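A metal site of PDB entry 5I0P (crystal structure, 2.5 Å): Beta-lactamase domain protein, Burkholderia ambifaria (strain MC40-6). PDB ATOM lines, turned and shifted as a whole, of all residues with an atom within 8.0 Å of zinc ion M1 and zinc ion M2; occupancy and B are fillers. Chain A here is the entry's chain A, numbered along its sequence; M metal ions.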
ATOM      1  N   LEU A  44     -15.606  39.165 -20.464  1.00  0.00           N
ATOM      2  CA  LEU A  44     -15.139  38.142 -21.380  1.00  0.00           C
ATOM      3  C   LEU A  44     -15.902  38.308 -22.685  1.00  0.00           C
ATOM      4  O   LEU A  44     -17.032  38.762 -22.669  1.00  0.00           O
ATOM      5  CB  LEU A  44     -15.337  36.726 -20.809  1.00  0.00           C
ATOM      6  CG  LEU A  44     -14.438  36.427 -19.605  1.00  0.00           C
ATOM      7  CD1 LEU A  44     -14.806  35.132 -18.989  1.00  0.00           C
ATOM      8  CD2 LEU A  44     -12.928  36.424 -19.956  1.00  0.00           C
ATOM      9  N   LEU A  48     -20.430  33.408 -22.203  1.00  0.00           N
ATOM     10  CA  LEU A  48     -20.071  33.654 -20.819  1.00  0.00           C
ATOM     11  C   LEU A  48     -19.329  34.995 -20.804  1.00  0.00           C
ATOM     12  O   LEU A  48     -18.198  35.070 -21.285  1.00  0.00           O
ATOM     13  CB  LEU A  48     -19.200  32.502 -20.335  1.00  0.00           C
ATOM     14  CG  LEU A  48     -18.794  32.438 -18.882  1.00  0.00           C
ATOM     15  CD1 LEU A  48     -19.929  31.936 -18.073  1.00  0.00           C
ATOM     16  CD2 LEU A  48     -17.541  31.552 -18.737  1.00  0.00           C
ATOM     17  N   HIS A  50     -18.315  37.201 -18.424  1.00  0.00           N
ATOM     18  CA  HIS A  50     -17.572  37.765 -17.317  1.00  0.00           C
ATOM     19  C   HIS A  50     -16.897  36.649 -16.544  1.00  0.00           C
ATOM     20  O   HIS A  50     -17.330  35.509 -16.556  1.00  0.00           O
ATOM     21  CB  HIS A  50     -18.505  38.550 -16.395  1.00  0.00           C
ATOM     22  CG  HIS A  50     -19.359  37.678 -15.544  1.00  0.00           C
ATOM     23  ND1 HIS A  50     -20.578  37.179 -15.980  1.00  0.00           N
ATOM     24  CD2 HIS A  50     -19.157  37.160 -14.304  1.00  0.00           C
ATOM     25  CE1 HIS A  50     -21.107  36.425 -15.023  1.00  0.00           C
ATOM     26  NE2 HIS A  50     -20.253  36.385 -14.008  1.00  0.00           N
ATOM     27  N   ILE A  51     -15.870  37.011 -15.793  1.00  0.00           N
ATOM     28  CA  ILE A  51     -15.343  36.139 -14.741  1.00  0.00           C
ATOM     29  C   ILE A  51     -15.106  36.990 -13.494  1.00  0.00           C
ATOM     30  O   ILE A  51     -14.654  38.131 -13.588  1.00  0.00           O
ATOM     31  CB  ILE A  51     -14.055  35.407 -15.181  1.00  0.00           C
ATOM     32  CG1 ILE A  51     -13.534  34.507 -14.046  1.00  0.00           C
ATOM     33  CG2 ILE A  51     -12.980  36.365 -15.710  1.00  0.00           C
ATOM     34  CD1 ILE A  51     -12.422  33.566 -14.453  1.00  0.00           C
ATOM     35  N   ASN A  52     -15.438  36.425 -12.340  1.00  0.00           N
ATOM     36  CA  ASN A  52     -15.194  37.070 -11.052  1.00  0.00           C
ATOM     37  C   ASN A  52     -13.822  36.663 -10.544  1.00  0.00           C
ATOM     38  O   ASN A  52     -13.513  35.475 -10.512  1.00  0.00           O
ATOM     39  CB  ASN A  52     -16.245  36.708 -10.017  1.00  0.00           C
ATOM     40  CG  ASN A  52     -17.633  37.019 -10.477  1.00  0.00           C
ATOM     41  OD1 ASN A  52     -17.864  38.104 -11.000  1.00  0.00           O
ATOM     42  ND2 ASN A  52     -18.583  36.104 -10.256  1.00  0.00           N
ATOM     43  N   ASP A  70      -7.220  33.835  -9.451  1.00  0.00           N
ATOM     44  CA  ASP A  70      -7.642  33.770 -10.855  1.00  0.00           C
ATOM     45  C   ASP A  70      -7.377  35.089 -11.580  1.00  0.00           C
ATOM     46  O   ASP A  70      -7.311  36.148 -10.970  1.00  0.00           O
ATOM     47  CB  ASP A  70      -9.113  33.335 -10.955  1.00  0.00           C
ATOM     48  CG  ASP A  70      -9.315  31.838 -10.631  1.00  0.00           C
ATOM     49  OD1 ASP A  70      -8.297  31.134 -10.532  1.00  0.00           O
ATOM     50  OD2 ASP A  70     -10.463  31.373 -10.490  1.00  0.00           O
ATOM     51  N   THR A 101      -7.587  28.608  -9.598  1.00  0.00           N
ATOM     52  CA  THR A 101      -8.472  27.499  -9.276  1.00  0.00           C
ATOM     53  C   THR A 101      -8.299  26.316 -10.223  1.00  0.00           C
ATOM     54  O   THR A 101      -8.393  25.147  -9.809  1.00  0.00           O
ATOM     55  CB  THR A 101      -9.933  27.983  -9.259  1.00  0.00           C
ATOM     56  OG1 THR A 101     -10.293  28.574 -10.519  1.00  0.00           O
ATOM     57  CG2 THR A 101     -10.180  28.976  -8.159  1.00  0.00           C
ATOM     58  N   HIS A 102      -8.100  26.586 -11.508  1.00  0.00           N
ATOM     59  CA  HIS A 102      -8.054  25.523 -12.492  1.00  0.00           C
ATOM     60  C   HIS A 102      -7.624  26.168 -13.805  1.00  0.00           C
ATOM     61  O   HIS A 102      -7.550  27.395 -13.920  1.00  0.00           O
ATOM     62  CB  HIS A 102      -9.388  24.776 -12.602  1.00  0.00           C
ATOM     63  CG  HIS A 102     -10.539  25.557 -13.178  1.00  0.00           C
ATOM     64  ND1 HIS A 102     -11.126  26.634 -12.536  1.00  0.00           N
ATOM     65  CD2 HIS A 102     -11.239  25.373 -14.321  1.00  0.00           C
ATOM     66  CE1 HIS A 102     -12.126  27.081 -13.262  1.00  0.00           C
ATOM     67  NE2 HIS A 102     -12.221  26.341 -14.353  1.00  0.00           N
ATOM     68  N   CYS A 103      -7.318  25.318 -14.798  1.00  0.00           N
ATOM     69  CA  CYS A 103      -6.525  25.768 -15.940  1.00  0.00           C
ATOM     70  C   CYS A 103      -7.339  26.354 -17.088  1.00  0.00           C
ATOM     71  O   CYS A 103      -6.755  26.687 -18.131  1.00  0.00           O
ATOM     72  CB  CYS A 103      -5.652  24.627 -16.475  1.00  0.00           C
ATOM     73  SG  CYS A 103      -6.579  23.295 -17.285  1.00  0.00           S
ATOM     74  N   HIS A 104      -8.665  26.456 -16.960  1.00  0.00           N
ATOM     75  CA  HIS A 104      -9.428  27.041 -18.069  1.00  0.00           C
ATOM     76  C   HIS A 104      -8.983  28.479 -18.320  1.00  0.00           C
ATOM     77  O   HIS A 104      -8.607  29.215 -17.380  1.00  0.00           O
ATOM     78  CB  HIS A 104     -10.933  26.962 -17.807  1.00  0.00           C
ATOM     79  CG  HIS A 104     -11.446  25.558 -17.878  1.00  0.00           C
ATOM     80  ND1 HIS A 104     -12.604  25.150 -17.244  1.00  0.00           N
ATOM     81  CD2 HIS A 104     -10.938  24.456 -18.463  1.00  0.00           C
ATOM     82  CE1 HIS A 104     -12.779  23.856 -17.450  1.00  0.00           C
ATOM     83  NE2 HIS A 104     -11.782  23.410 -18.184  1.00  0.00           N
ATOM     84  N   PRO A 105      -8.992  28.886 -19.589  1.00  0.00           N
ATOM     85  CA  PRO A 105      -8.288  30.126 -19.987  1.00  0.00           C
ATOM     86  C   PRO A 105      -8.765  31.390 -19.245  1.00  0.00           C
ATOM     87  O   PRO A 105      -7.958  32.305 -19.005  1.00  0.00           O
ATOM     88  CB  PRO A 105      -8.588  30.216 -21.480  1.00  0.00           C
ATOM     89  CG  PRO A 105      -9.025  28.889 -21.864  1.00  0.00           C
ATOM     90  CD  PRO A 105      -9.689  28.266 -20.710  1.00  0.00           C
ATOM     91  N   ASP A 106     -10.064  31.476 -18.919  1.00  0.00           N
ATOM     92  CA  ASP A 106     -10.533  32.669 -18.239  1.00  0.00           C
ATOM     93  C   ASP A 106      -9.998  32.749 -16.804  1.00  0.00           C
ATOM     94  O   ASP A 106      -9.940  33.849 -16.246  1.00  0.00           O
ATOM     95  CB  ASP A 106     -12.083  32.766 -18.307  1.00  0.00           C
ATOM     96  CG  ASP A 106     -12.816  31.450 -17.969  1.00  0.00           C
ATOM     97  OD1 ASP A 106     -13.874  31.510 -17.281  1.00  0.00           O
ATOM     98  OD2 ASP A 106     -12.372  30.358 -18.388  1.00  0.00           O
ATOM     99  N   HIS A 107      -9.535  31.623 -16.222  1.00  0.00           N
ATOM    100  CA  HIS A 107      -8.949  31.674 -14.883  1.00  0.00           C
ATOM    101  C   HIS A 107      -7.437  31.813 -14.889  1.00  0.00           C
ATOM    102  O   HIS A 107      -6.895  32.471 -13.996  1.00  0.00           O
ATOM    103  CB  HIS A 107      -9.348  30.425 -14.096  1.00  0.00           C
ATOM    104  CG  HIS A 107     -10.824  30.275 -13.967  1.00  0.00           C
ATOM    105  ND1 HIS A 107     -11.510  30.516 -12.788  1.00  0.00           N
ATOM    106  CD2 HIS A 107     -11.774  29.963 -14.885  1.00  0.00           C
ATOM    107  CE1 HIS A 107     -12.792  30.319 -12.976  1.00  0.00           C
ATOM    108  NE2 HIS A 107     -12.982  29.981 -14.232  1.00  0.00           N
ATOM    109  N   GLU A 133      -4.036  20.673 -12.728  1.00  0.00           N
ATOM    110  CA  GLU A 133      -4.398  21.840 -13.525  1.00  0.00           C
ATOM    111  C   GLU A 133      -3.173  22.474 -14.153  1.00  0.00           C
ATOM    112  O   GLU A 133      -3.172  22.775 -15.351  1.00  0.00           O
ATOM    113  CB  GLU A 133      -5.140  22.863 -12.655  1.00  0.00           C
ATOM    114  CG  GLU A 133      -6.410  22.318 -12.015  1.00  0.00           C
ATOM    115  CD  GLU A 133      -7.519  22.104 -13.041  1.00  0.00           C
ATOM    116  OE1 GLU A 133      -7.427  22.703 -14.143  1.00  0.00           O
ATOM    117  OE2 GLU A 133      -8.493  21.361 -12.739  1.00  0.00           O
ATOM    118  N   HIS A 213     -15.131  18.696 -14.080  1.00  0.00           N
ATOM    119  CA  HIS A 213     -15.026  19.926 -14.872  1.00  0.00           C
ATOM    120  C   HIS A 213     -13.618  20.124 -15.425  1.00  0.00           C
ATOM    121  O   HIS A 213     -13.448  20.563 -16.562  1.00  0.00           O
ATOM    122  CB  HIS A 213     -15.483  21.107 -14.013  1.00  0.00           C
ATOM    123  CG  HIS A 213     -15.344  22.435 -14.688  1.00  0.00           C
ATOM    124  ND1 HIS A 213     -16.111  22.810 -15.774  1.00  0.00           N
ATOM    125  CD2 HIS A 213     -14.573  23.507 -14.377  1.00  0.00           C
ATOM    126  CE1 HIS A 213     -15.766  24.033 -16.140  1.00  0.00           C
ATOM    127  NE2 HIS A 213     -14.854  24.484 -15.311  1.00  0.00           N
ATOM    128  N   SER A 214     -12.612  19.744 -14.654  1.00  0.00           N
ATOM    129  CA  SER A 214     -11.199  19.959 -14.977  1.00  0.00           C
ATOM    130  C   SER A 214     -10.390  18.946 -14.183  1.00  0.00           C
ATOM    131  O   SER A 214     -10.937  18.262 -13.299  1.00  0.00           O
ATOM    132  CB  SER A 214     -10.770  21.394 -14.650  1.00  0.00           C
ATOM    133  OG  SER A 214     -10.921  21.677 -13.268  1.00  0.00           O
ATOM    134  N   HIS A 217      -9.709  20.558  -9.753  1.00  0.00           N
ATOM    135  CA  HIS A 217     -10.167  21.924  -9.561  1.00  0.00           C
ATOM    136  C   HIS A 217     -10.002  22.355  -8.116  1.00  0.00           C
ATOM    137  O   HIS A 217     -10.389  21.642  -7.186  1.00  0.00           O
ATOM    138  CB  HIS A 217     -11.634  22.036  -9.990  1.00  0.00           C
ATOM    139  CG  HIS A 217     -12.214  23.404  -9.806  1.00  0.00           C
ATOM    140  ND1 HIS A 217     -12.586  23.889  -8.562  1.00  0.00           N
ATOM    141  CD2 HIS A 217     -12.513  24.372 -10.705  1.00  0.00           C
ATOM    142  CE1 HIS A 217     -13.063  25.116  -8.712  1.00  0.00           C
ATOM    143  NE2 HIS A 217     -13.047  25.426  -9.994  1.00  0.00           N
ATOM    144  N   GLY A 231     -14.902  28.619  -7.522  1.00  0.00           N
ATOM    145  CA  GLY A 231     -14.409  28.387  -8.876  1.00  0.00           C
ATOM    146  C   GLY A 231     -15.577  28.177  -9.817  1.00  0.00           C
ATOM    147  O   GLY A 231     -16.589  28.889  -9.758  1.00  0.00           O
ATOM    148  N   ASP A 232     -15.478  27.177 -10.672  1.00  0.00           N
ATOM    149  CA  ASP A 232     -16.578  26.831 -11.553  1.00  0.00           C
ATOM    150  C   ASP A 232     -17.384  25.641 -11.033  1.00  0.00           C
ATOM    151  O   ASP A 232     -18.277  25.184 -11.736  1.00  0.00           O
ATOM    152  CB  ASP A 232     -16.087  26.490 -12.950  1.00  0.00           C
ATOM    153  CG  ASP A 232     -15.630  27.689 -13.754  1.00  0.00           C
ATOM    154  OD1 ASP A 232     -15.738  28.863 -13.374  1.00  0.00           O
ATOM    155  OD2 ASP A 232     -15.118  27.423 -14.849  1.00  0.00           O
ATOM    156  N   MET A 233     -17.097  25.128  -9.827  1.00  0.00           N
ATOM    157  CA  MET A 233     -17.778  23.909  -9.400  1.00  0.00           C
ATOM    158  C   MET A 233     -19.224  24.190  -8.994  1.00  0.00           C
ATOM    159  O   MET A 233     -20.115  23.359  -9.258  1.00  0.00           O
ATOM    160  CB  MET A 233     -17.010  23.226  -8.256  1.00  0.00           C
ATOM    161  CG  MET A 233     -15.695  22.681  -8.700  1.00  0.00           C
ATOM    162  SD  MET A 233     -15.870  21.298  -9.859  1.00  0.00           S
ATOM    163  CE  MET A 233     -16.641  20.031  -8.848  1.00  0.00           C
ATOM    164  N   LEU A 235     -21.891  27.212  -9.618  1.00  0.00           N
ATOM    165  CA  LEU A 235     -22.241  28.496 -10.164  1.00  0.00           C
ATOM    166  C   LEU A 235     -23.743  28.759  -9.948  1.00  0.00           C
ATOM    167  O   LEU A 235     -24.557  27.848 -10.086  1.00  0.00           O
ATOM    168  CB  LEU A 235     -21.903  28.571 -11.649  1.00  0.00           C
ATOM    169  CG  LEU A 235     -20.453  28.213 -11.956  1.00  0.00           C
ATOM    170  CD1 LEU A 235     -20.245  28.057 -13.483  1.00  0.00           C
ATOM    171  CD2 LEU A 235     -19.520  29.216 -11.387  1.00  0.00           C
ATOM    172  N   ILE A 238     -25.647  29.250 -13.902  1.00  0.00           N
ATOM    173  CA  ILE A 238     -25.399  28.401 -15.056  1.00  0.00           C
ATOM    174  C   ILE A 238     -24.844  27.066 -14.575  1.00  0.00           C
ATOM    175  O   ILE A 238     -24.258  26.962 -13.502  1.00  0.00           O
ATOM    176  CB  ILE A 238     -24.438  29.061 -16.047  1.00  0.00           C
ATOM    177  CG1 ILE A 238     -23.054  29.148 -15.468  1.00  0.00           C
ATOM    178  CG2 ILE A 238     -24.874  30.507 -16.338  1.00  0.00           C
ATOM    179  CD1 ILE A 238     -22.099  29.848 -16.381  1.00  0.00           C
ATOM    180  N   THR A 240     -22.259  23.800 -14.628  1.00  0.00           N
ATOM    181  CA  THR A 240     -20.830  23.636 -14.834  1.00  0.00           C
ATOM    182  C   THR A 240     -20.579  22.736 -16.036  1.00  0.00           C
ATOM    183  O   THR A 240     -21.212  21.675 -16.161  1.00  0.00           O
ATOM    184  CB  THR A 240     -20.183  23.018 -13.587  1.00  0.00           C
ATOM    185  OG1 THR A 240     -20.354  23.902 -12.475  1.00  0.00           O
ATOM    186  CG2 THR A 240     -18.726  22.725 -13.813  1.00  0.00           C
ATOM    187  N   ASN A 241     -19.694  23.153 -16.936  1.00  0.00           N
ATOM    188  CA  ASN A 241     -19.401  22.313 -18.086  1.00  0.00           C
ATOM    189  C   ASN A 241     -18.752  21.000 -17.664  1.00  0.00           C
ATOM    190  O   ASN A 241     -17.818  20.980 -16.858  1.00  0.00           O
ATOM    191  CB  ASN A 241     -18.497  23.004 -19.088  1.00  0.00           C
ATOM    192  CG  ASN A 241     -18.164  22.060 -20.234  1.00  0.00           C
ATOM    193  OD1 ASN A 241     -19.015  21.812 -21.091  1.00  0.00           O
ATOM    194  ND2 ASN A 241     -16.964  21.484 -20.221  1.00  0.00           N
ATOM    195  N   PRO A 275     -18.628  32.622  -6.510  1.00  0.00           N
ATOM    196  CA  PRO A 275     -18.456  31.851  -7.732  1.00  0.00           C
ATOM    197  C   PRO A 275     -17.779  32.696  -8.795  1.00  0.00           C
ATOM    198  O   PRO A 275     -17.836  33.927  -8.794  1.00  0.00           O
ATOM    199  CB  PRO A 275     -19.895  31.550  -8.154  1.00  0.00           C
ATOM    200  CG  PRO A 275     -20.599  32.900  -7.773  1.00  0.00           C
ATOM    201  CD  PRO A 275     -19.893  33.389  -6.507  1.00  0.00           C
ATOM    202  N   SER A 276     -17.139  32.001  -9.737  1.00  0.00           N
ATOM    203  CA  SER A 276     -16.402  32.718 -10.754  1.00  0.00           C
ATOM    204  C   SER A 276     -17.299  33.319 -11.826  1.00  0.00           C
ATOM    205  O   SER A 276     -16.830  34.129 -12.614  1.00  0.00           O
ATOM    206  CB  SER A 276     -15.339  31.815 -11.342  1.00  0.00           C
ATOM    207  OG  SER A 276     -14.356  31.635 -10.318  1.00  0.00           O
ATOM    208  N   HIS A 277     -18.572  32.936 -11.873  1.00  0.00           N
ATOM    209  CA  HIS A 277     -19.537  33.504 -12.804  1.00  0.00           C
ATOM    210  C   HIS A 277     -20.878  33.603 -12.097  1.00  0.00           C
ATOM    211  O   HIS A 277     -21.309  32.629 -11.474  1.00  0.00           O
ATOM    212  CB  HIS A 277     -19.622  32.677 -14.101  1.00  0.00           C
ATOM    213  CG  HIS A 277     -18.278  32.290 -14.651  1.00  0.00           C
ATOM    214  ND1 HIS A 277     -17.551  33.095 -15.497  1.00  0.00           N
ATOM    215  CD2 HIS A 277     -17.532  31.170 -14.475  1.00  0.00           C
ATOM    216  CE1 HIS A 277     -16.418  32.489 -15.823  1.00  0.00           C
ATOM    217  NE2 HIS A 277     -16.383  31.326 -15.206  1.00  0.00           N
HETATM  218 ZN    ZN M   1     -13.857  26.357 -16.125  1.00  0.00          ZN
HETATM  219 ZN    ZN M   2     -14.827  29.704 -15.566  1.00  0.00          ZN
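The side-chain hydroxyl of Thr 101 sits at hydrogen-bond distance from a ring nitrogen (ND1) of His 102, 2.9 Å away.
A ring nitrogen (ND1) of His 107 sits at hydrogen-bond distance from the side-chain hydroxyl of Thr 101, at 3.2 Å.
A ring nitrogen (NE2) of His 217 lies within hydrogen-bond range of the backbone NH (N) of Asp 232, at 3.1 Å.
ND1 of His 277 is in hydrogen-bond range of O of His 50 (2.6 Å).
A ring nitrogen (ND1) of His 213 lies within hydrogen-bond range of the backbone carbonyl oxygen of Asn 241, at 2.7 Å.
The side-chain hydroxyl (OG1) of Thr 240 is in hydrogen-bond range of the backbone carbonyl oxygen (O) of Asp 232.
A ring nitrogen (NE2) of His 277 sits close to the side-chain carboxylate (OD1) of Asp 106, 3.3 Å away.
ND1 of His 102 sits close to NE2 of His 217.
NE2 of His 277 binds zinc ion M2 (2.3 Å).
NE2 of His 107 is bound to zinc ion M2, at 2.3 Å.
OD2 of Asp 232 is bound to zinc ion M2, 2.4 Å away.
Zinc ion M2 is bound by OD1 of Asp 232, at 2.5 Å.
Slightly farther from zinc ion M2 lies the side-chain carboxylate (OD1) of Asp 106 (2.7 Å).
Of the 27 residues printed, 4 come within 4 Å of zinc ion M2.
Along chain A the residues within 4 Å of zinc ion M2 span positions 106 to 277.
Zinc ion M1 is bound by a ring nitrogen (ND1) of His 104 (2.1 Å), the side-chain carboxylate (OD2) of Asp 232 (2.1 Å), a ring nitrogen (NE2) of His 213 (2.3 Å) and a ring nitrogen (NE2) of His 102 (2.4 Å).
Four residues have an atom within 4 Å of zinc ion M1: His 102, His 104, His 213 and Asp 232.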
